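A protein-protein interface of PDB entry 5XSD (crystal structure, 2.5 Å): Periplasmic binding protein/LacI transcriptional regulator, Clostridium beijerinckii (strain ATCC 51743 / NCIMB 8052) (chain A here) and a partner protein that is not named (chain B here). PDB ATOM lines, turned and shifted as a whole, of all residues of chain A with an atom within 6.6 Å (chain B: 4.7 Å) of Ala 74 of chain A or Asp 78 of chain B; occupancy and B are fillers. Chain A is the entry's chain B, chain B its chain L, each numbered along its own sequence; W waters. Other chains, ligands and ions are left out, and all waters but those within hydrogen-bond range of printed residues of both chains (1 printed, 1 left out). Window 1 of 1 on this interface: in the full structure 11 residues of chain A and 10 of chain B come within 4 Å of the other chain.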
ATOM      1  N   LYS A  20       3.798 -23.875   9.702  1.00  0.00           N
ATOM      2  CA  LYS A  20       2.643 -23.128  10.164  1.00  0.00           C
ATOM      3  C   LYS A  20       3.066 -21.834  10.785  1.00  0.00           C
ATOM      4  O   LYS A  20       3.941 -21.810  11.651  1.00  0.00           O
ATOM      5  CB  LYS A  20       1.808 -23.895  11.190  1.00  0.00           C
ATOM      6  CG  LYS A  20       0.574 -23.084  11.599  1.00  0.00           C
ATOM      7  CD  LYS A  20      -0.241 -23.730  12.718  1.00  0.00           C
ATOM      8  CE  LYS A  20      -1.221 -24.769  12.189  1.00  0.00           C
ATOM      9  NZ  LYS A  20      -2.472 -24.724  12.989  1.00  0.00           N
ATOM     10  N   GLU A  52      -2.356 -19.659  10.290  1.00  0.00           N
ATOM     11  CA  GLU A  52      -3.488 -19.732  11.202  1.00  0.00           C
ATOM     12  C   GLU A  52      -3.758 -18.372  11.825  1.00  0.00           C
ATOM     13  O   GLU A  52      -2.926 -17.809  12.572  1.00  0.00           O
ATOM     14  CB  GLU A  52      -3.260 -20.770  12.307  1.00  0.00           C
ATOM     15  CG  GLU A  52      -4.561 -21.316  12.887  1.00  0.00           C
ATOM     16  CD  GLU A  52      -4.345 -22.265  14.064  1.00  0.00           C
ATOM     17  OE1 GLU A  52      -3.191 -22.669  14.340  1.00  0.00           O
ATOM     18  OE2 GLU A  52      -5.341 -22.576  14.739  1.00  0.00           O
ATOM     19  N   ASP A  69       0.849 -17.815  23.905  1.00  0.00           N
ATOM     20  CA  ASP A  69       1.325 -18.933  24.710  1.00  0.00           C
ATOM     21  C   ASP A  69       1.051 -20.300  24.042  1.00  0.00           C
ATOM     22  O   ASP A  69       1.967 -21.131  23.928  1.00  0.00           O
ATOM     23  CB  ASP A  69       0.680 -18.864  26.097  1.00  0.00           C
ATOM     24  CG  ASP A  69       1.613 -19.329  27.197  1.00  0.00           C
ATOM     25  OD1 ASP A  69       2.650 -18.664  27.411  1.00  0.00           O
ATOM     26  OD2 ASP A  69       1.303 -20.352  27.851  1.00  0.00           O
ATOM     27  N   MET A  70      -0.187 -20.527  23.593  1.00  0.00           N
ATOM     28  CA  MET A  70      -0.536 -21.725  22.813  1.00  0.00           C
ATOM     29  C   MET A  70       0.281 -21.868  21.526  1.00  0.00           C
ATOM     30  O   MET A  70       0.700 -22.967  21.165  1.00  0.00           O
ATOM     31  CB  MET A  70      -2.011 -21.713  22.418  1.00  0.00           C
ATOM     32  CG  MET A  70      -2.981 -21.588  23.553  1.00  0.00           C
ATOM     33  SD  MET A  70      -4.663 -21.796  22.934  1.00  0.00           S
ATOM     34  CE  MET A  70      -4.419 -23.208  21.851  1.00  0.00           C
ATOM     35  N   ALA A  71       0.477 -20.761  20.814  1.00  0.00           N
ATOM     36  CA  ALA A  71       1.286 -20.796  19.603  1.00  0.00           C
ATOM     37  C   ALA A  71       2.704 -21.257  19.942  1.00  0.00           C
ATOM     38  O   ALA A  71       3.283 -22.097  19.235  1.00  0.00           O
ATOM     39  CB  ALA A  71       1.302 -19.433  18.924  1.00  0.00           C
ATOM     40  N   THR A  72       3.249 -20.724  21.035  1.00  0.00           N
ATOM     41  CA  THR A  72       4.580 -21.111  21.490  1.00  0.00           C
ATOM     42  C   THR A  72       4.598 -22.591  21.865  1.00  0.00           C
ATOM     43  O   THR A  72       5.499 -23.330  21.475  1.00  0.00           O
ATOM     44  CB  THR A  72       5.033 -20.253  22.693  1.00  0.00           C
ATOM     45  OG1 THR A  72       5.121 -18.875  22.302  1.00  0.00           O
ATOM     46  CG2 THR A  72       6.384 -20.710  23.226  1.00  0.00           C
ATOM     47  N   SER A  73       3.584 -23.026  22.604  1.00  0.00           N
ATOM     48  CA  SER A  73       3.513 -24.415  23.050  1.00  0.00           C
ATOM     49  C   SER A  73       3.387 -25.399  21.880  1.00  0.00           C
ATOM     50  O   SER A  73       3.920 -26.513  21.946  1.00  0.00           O
ATOM     51  CB  SER A  73       2.334 -24.604  24.026  1.00  0.00           C
ATOM     52  OG  SER A  73       2.573 -23.920  25.249  1.00  0.00           O
ATOM     53  N   ALA A  74       2.687 -25.001  20.818  1.00  0.00           N
ATOM     54  CA  ALA A  74       2.480 -25.900  19.668  1.00  0.00           C
ATOM     55  C   ALA A  74       3.697 -25.933  18.714  1.00  0.00           C
ATOM     56  O   ALA A  74       3.692 -26.626  17.694  1.00  0.00           O
ATOM     57  CB  ALA A  74       1.192 -25.501  18.902  1.00  0.00           C
ATOM     58  N   LYS A  75       4.737 -25.181  19.075  1.00  0.00           N
ATOM     59  CA  LYS A  75       6.001 -25.121  18.318  1.00  0.00           C
ATOM     60  C   LYS A  75       5.808 -24.844  16.820  1.00  0.00           C
ATOM     61  O   LYS A  75       6.409 -25.491  15.962  1.00  0.00           O
ATOM     62  CB  LYS A  75       6.794 -26.407  18.531  1.00  0.00           C
ATOM     63  CG  LYS A  75       7.172 -26.610  20.003  1.00  0.00           C
ATOM     64  CD  LYS A  75       7.963 -27.873  20.222  1.00  0.00           C
ATOM     65  CE  LYS A  75       8.302 -28.053  21.698  1.00  0.00           C
ATOM     66  NZ  LYS A  75       9.097 -29.295  21.915  1.00  0.00           N
ATOM     67  N   VAL A  76       4.966 -23.856  16.523  1.00  0.00           N
ATOM     68  CA  VAL A  76       4.704 -23.458  15.154  1.00  0.00           C
ATOM     69  C   VAL A  76       5.974 -22.831  14.575  1.00  0.00           C
ATOM     70  O   VAL A  76       6.906 -22.501  15.306  1.00  0.00           O
ATOM     71  CB  VAL A  76       3.515 -22.505  15.088  1.00  0.00           C
ATOM     72  CG1 VAL A  76       2.256 -23.244  15.554  1.00  0.00           C
ATOM     73  CG2 VAL A  76       3.773 -21.250  15.954  1.00  0.00           C
ATOM     74  N   SER A  77       6.043 -22.710  13.258  1.00  0.00           N
ATOM     75  CA  SER A  77       7.305 -22.298  12.640  1.00  0.00           C
ATOM     76  C   SER A  77       7.582 -20.811  12.868  1.00  0.00           C
ATOM     77  O   SER A  77       8.725 -20.385  12.865  1.00  0.00           O
ATOM     78  CB  SER A  77       7.300 -22.642  11.157  1.00  0.00           C
ATOM     79  OG  SER A  77       7.247 -24.052  10.991  1.00  0.00           O
ATOM     80  N   ILE A 101      11.565 -19.958  17.915  1.00  0.00           N
ATOM     81  CA  ILE A 101      10.409 -19.525  17.127  1.00  0.00           C
ATOM     82  C   ILE A 101      10.573 -18.044  16.746  1.00  0.00           C
ATOM     83  O   ILE A 101      10.538 -17.179  17.611  1.00  0.00           O
ATOM     84  CB  ILE A 101       9.075 -19.672  17.899  1.00  0.00           C
ATOM     85  CG1 ILE A 101       8.892 -21.086  18.443  1.00  0.00           C
ATOM     86  CG2 ILE A 101       7.890 -19.208  17.031  1.00  0.00           C
ATOM     87  CD1 ILE A 101       7.610 -21.240  19.210  1.00  0.00           C
ATOM     88  N   TYR B  74      -2.307 -31.197  10.444  1.00  0.00           N
ATOM     89  CA  TYR B  74      -1.912 -29.928  11.070  1.00  0.00           C
ATOM     90  C   TYR B  74      -2.368 -29.852  12.536  1.00  0.00           C
ATOM     91  O   TYR B  74      -1.576 -29.511  13.419  1.00  0.00           O
ATOM     92  CB  TYR B  74      -2.451 -28.735  10.264  1.00  0.00           C
ATOM     93  CG  TYR B  74      -1.721 -28.565   8.948  1.00  0.00           C
ATOM     94  CD1 TYR B  74      -0.486 -27.930   8.896  1.00  0.00           C
ATOM     95  CD2 TYR B  74      -2.245 -29.078   7.760  1.00  0.00           C
ATOM     96  CE1 TYR B  74       0.204 -27.791   7.691  1.00  0.00           C
ATOM     97  CE2 TYR B  74      -1.559 -28.951   6.552  1.00  0.00           C
ATOM     98  CZ  TYR B  74      -0.336 -28.306   6.524  1.00  0.00           C
ATOM     99  OH  TYR B  74       0.356 -28.171   5.339  1.00  0.00           O
ATOM    100  N   ILE B  75      -3.627 -30.180  12.801  1.00  0.00           N
ATOM    101  CA  ILE B  75      -4.093 -30.252  14.184  1.00  0.00           C
ATOM    102  C   ILE B  75      -3.272 -31.253  14.999  1.00  0.00           C
ATOM    103  O   ILE B  75      -2.889 -30.985  16.143  1.00  0.00           O
ATOM    104  CB  ILE B  75      -5.559 -30.649  14.260  1.00  0.00           C
ATOM    105  CG1 ILE B  75      -6.372 -29.852  13.230  1.00  0.00           C
ATOM    106  CG2 ILE B  75      -6.068 -30.436  15.679  1.00  0.00           C
ATOM    107  CD1 ILE B  75      -7.693 -30.506  12.849  1.00  0.00           C
ATOM    108  N   LEU B  76      -2.986 -32.395  14.389  1.00  0.00           N
ATOM    109  CA  LEU B  76      -2.263 -33.464  15.062  1.00  0.00           C
ATOM    110  C   LEU B  76      -0.834 -33.070  15.401  1.00  0.00           C
ATOM    111  O   LEU B  76      -0.313 -33.472  16.451  1.00  0.00           O
ATOM    112  CB  LEU B  76      -2.259 -34.737  14.206  1.00  0.00           C
ATOM    113  CG  LEU B  76      -3.470 -35.654  14.437  1.00  0.00           C
ATOM    114  CD1 LEU B  76      -3.472 -36.800  13.433  1.00  0.00           C
ATOM    115  CD2 LEU B  76      -3.483 -36.180  15.876  1.00  0.00           C
ATOM    116  N   ARG B  77      -0.201 -32.297  14.516  1.00  0.00           N
ATOM    117  CA  ARG B  77       1.163 -31.843  14.762  1.00  0.00           C
ATOM    118  C   ARG B  77       1.169 -30.879  15.930  1.00  0.00           C
ATOM    119  O   ARG B  77       2.046 -30.948  16.794  1.00  0.00           O
ATOM    120  CB  ARG B  77       1.785 -31.168  13.536  1.00  0.00           C
ATOM    121  CG  ARG B  77       3.168 -30.583  13.830  1.00  0.00           C
ATOM    122  CD  ARG B  77       3.820 -29.962  12.592  1.00  0.00           C
ATOM    123  NE  ARG B  77       2.991 -28.921  11.981  1.00  0.00           N
ATOM    124  CZ  ARG B  77       3.289 -28.296  10.844  1.00  0.00           C
ATOM    125  NH1 ARG B  77       4.399 -28.604  10.183  1.00  0.00           N
ATOM    126  NH2 ARG B  77       2.477 -27.367  10.365  1.00  0.00           N
ATOM    127  N   ASP B  78       0.176 -29.995  15.966  1.00  0.00           N
ATOM    128  CA  ASP B  78       0.074 -29.038  17.062  1.00  0.00           C
ATOM    129  C   ASP B  78      -0.226 -29.755  18.367  1.00  0.00           C
ATOM    130  O   ASP B  78       0.362 -29.443  19.400  1.00  0.00           O
ATOM    131  CB  ASP B  78      -0.991 -27.980  16.768  1.00  0.00           C
ATOM    132  CG  ASP B  78      -0.605 -27.087  15.609  1.00  0.00           C
ATOM    133  OD1 ASP B  78       0.615 -26.999  15.312  1.00  0.00           O
ATOM    134  OD2 ASP B  78      -1.518 -26.488  14.997  1.00  0.00           O
ATOM    135  N   LEU B  79      -1.141 -30.715  18.309  1.00  0.00           N
ATOM    136  CA  LEU B  79      -1.456 -31.529  19.469  1.00  0.00           C
ATOM    137  C   LEU B  79      -0.204 -32.256  19.953  1.00  0.00           C
ATOM    138  O   LEU B  79       0.141 -32.201  21.143  1.00  0.00           O
ATOM    139  CB  LEU B  79      -2.562 -32.527  19.143  1.00  0.00           C
ATOM    140  CG  LEU B  79      -2.923 -33.481  20.276  1.00  0.00           C
ATOM    141  CD1 LEU B  79      -3.208 -32.688  21.557  1.00  0.00           C
ATOM    142  CD2 LEU B  79      -4.123 -34.345  19.882  1.00  0.00           C
ATOM    143  N   ASP B  80       0.488 -32.916  19.027  1.00  0.00           N
ATOM    144  CA  ASP B  80       1.664 -33.705  19.398  1.00  0.00           C
ATOM    145  C   ASP B  80       2.738 -32.792  20.015  1.00  0.00           C
ATOM    146  O   ASP B  80       3.315 -33.117  21.062  1.00  0.00           O
ATOM    147  CB  ASP B  80       2.206 -34.475  18.181  1.00  0.00           C
ATOM    148  CG  ASP B  80       3.236 -35.539  18.556  1.00  0.00           C
ATOM    149  OD1 ASP B  80       3.303 -35.961  19.738  1.00  0.00           O
ATOM    150  OD2 ASP B  80       3.988 -35.959  17.655  1.00  0.00           O
ATOM    151  N   ASN B  81       2.975 -31.635  19.392  1.00  0.00           N
ATOM    152  CA  ASN B  81       3.957 -30.685  19.906  1.00  0.00           C
ATOM    153  C   ASN B  81       3.542 -30.072  21.244  1.00  0.00           C
ATOM    154  O   ASN B  81       4.396 -29.817  22.099  1.00  0.00           O
ATOM    155  CB  ASN B  81       4.216 -29.561  18.893  1.00  0.00           C
ATOM    156  CG  ASN B  81       5.158 -29.976  17.765  1.00  0.00           C
ATOM    157  OD1 ASN B  81       6.134 -30.718  17.970  1.00  0.00           O
ATOM    158  ND2 ASN B  81       4.868 -29.491  16.564  1.00  0.00           N
ATOM    159  N   THR B  82       2.244 -29.840  21.436  1.00  0.00           N
ATOM    160  CA  THR B  82       1.769 -29.236  22.687  1.00  0.00           C
ATOM    161  C   THR B  82       1.998 -30.216  23.841  1.00  0.00           C
ATOM    162  O   THR B  82       2.567 -29.847  24.870  1.00  0.00           O
ATOM    163  CB  THR B  82       0.286 -28.815  22.593  1.00  0.00           C
ATOM    164  OG1 THR B  82       0.135 -27.876  21.517  1.00  0.00           O
ATOM    165  CG2 THR B  82      -0.183 -28.145  23.898  1.00  0.00           C
ATOM    166  N   TYR B 123      -6.780 -28.625  21.308  1.00  0.00           N
ATOM    167  CA  TYR B 123      -6.472 -29.313  20.056  1.00  0.00           C
ATOM    168  C   TYR B 123      -7.207 -30.634  19.914  1.00  0.00           C
ATOM    169  O   TYR B 123      -7.538 -31.046  18.806  1.00  0.00           O
ATOM    170  CB  TYR B 123      -4.975 -29.562  19.938  1.00  0.00           C
ATOM    171  CG  TYR B 123      -4.212 -28.290  19.799  1.00  0.00           C
ATOM    172  CD1 TYR B 123      -4.317 -27.531  18.638  1.00  0.00           C
ATOM    173  CD2 TYR B 123      -3.398 -27.828  20.824  1.00  0.00           C
ATOM    174  CE1 TYR B 123      -3.632 -26.349  18.501  1.00  0.00           C
ATOM    175  CE2 TYR B 123      -2.706 -26.637  20.696  1.00  0.00           C
ATOM    176  CZ  TYR B 123      -2.833 -25.904  19.532  1.00  0.00           C
ATOM    177  OH  TYR B 123      -2.150 -24.722  19.382  1.00  0.00           O
HETATM  178  O   HOH W   1      -0.506 -24.824  22.537  1.00  0.00           O
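The side-chain amino group of Lys 20 of chain A lies within salt-bridge range of the side-chain carboxylate of Asp 78 of chain B, 2.8 Å away. The side-chain amide nitrogen (ND2) of Asn 81 of chain B lies close to the backbone carbonyl oxygen (O) of Ala 74 of chain A, 3.3 Å away. The backbone carbonyl oxygen of Ser 73 of chain A sits close to the backbone carbonyl oxygen of Asn 81 of chain B (3.3 Å).
The side-chain amino group (NZ) of Lys 20 of chain A is in salt-bridge range of the side-chain carboxylate (OE1) of Glu 52 of chain A. The backbone carbonyl oxygen of Lys 20 of chain A lies within hydrogen-bond range of the backbone NH of Ser 77 of chain A, at 2.8 Å. O of Asp 69 of chain A sits at hydrogen-bond distance from OG of Ser 73 of chain A. The backbone carbonyl oxygen (O) of Arg 77 of chain B is in hydrogen-bond range of the side-chain amide nitrogen (ND2) of Asn 81 of chain B, at 3.2 Å. The side-chain hydroxyl (OG1) of Thr 82 of chain B lies within hydrogen-bond range of the backbone carbonyl oxygen (O) of Asp 78 of chain B (2.6 Å).
Among the printed residues, merely in contact across the chains: Ala 74 of chain A with Tyr 123 of chain B (3.5 Å), Ser 73 of chain A with Thr 82 of chain B (3.5 Å), Ala 74 of chain A with Thr 82 of chain B (3.6 Å), Lys 20 of chain A with Arg 77 of chain B (3.6 Å), Met 70 of chain A with Tyr 123 of chain B (3.7 Å) and Ala 74 of chain A with Asp 78 of chain B (3.9 Å).
Ala 74 of chain A touches just these residues of chain B: Asp 78, Asn 81, Thr 82 and Tyr 123. Asp 78 of chain B touches just these residues of chain A: Lys 20 (2.8 Å) and Ala 74 (3.9 Å). Of the printed residues of chain B, Met 70 of chain A touches Tyr 123 (3.7 Å). Of the printed residues of chain B, Lys 20 of chain A touches Arg 77 (3.6 Å) and Asp 78 (2.8 Å). Of the printed residues of chain B, Ser 73 of chain A touches Asn 81 (3.3 Å) and Thr 82 (3.5 Å). Of the printed residues of chain A, Asn 81 of chain B touches Ser 73 and Ala 74. Printed residues of chain A within 4 Å of Thr 82 of chain B: Ser 73 (3.5 Å) and Ala 74 (3.6 Å). The nearest residue of chain A that does not touch Asp 78 of chain B is Val 76 of chain A (4.1 Å). The nearest printed residue of chain A that does not touch Asn 81 of chain B is Lys 75 of chain A (4.0001 Å).
Of the 10 printed residues of chain B, 5 touch a printed residue of chain A. Hydrophobic or aromatic side chains of chain B within 4 Å of the printed part of chain A: Tyr 123. Along chain B the printed residues that touch a printed residue of chain A span positions 77 to 123. Among the printed residues, Asp or Glu carboxylates within 4 Å of a Lys or Arg side-chain nitrogen of the other chain: Lys 20 of chain A with Asp 78 of chain B.
Water W1 lies within hydrogen-bond range of O of Met 70 of chain A and OG1 of Thr 82 of chain B.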
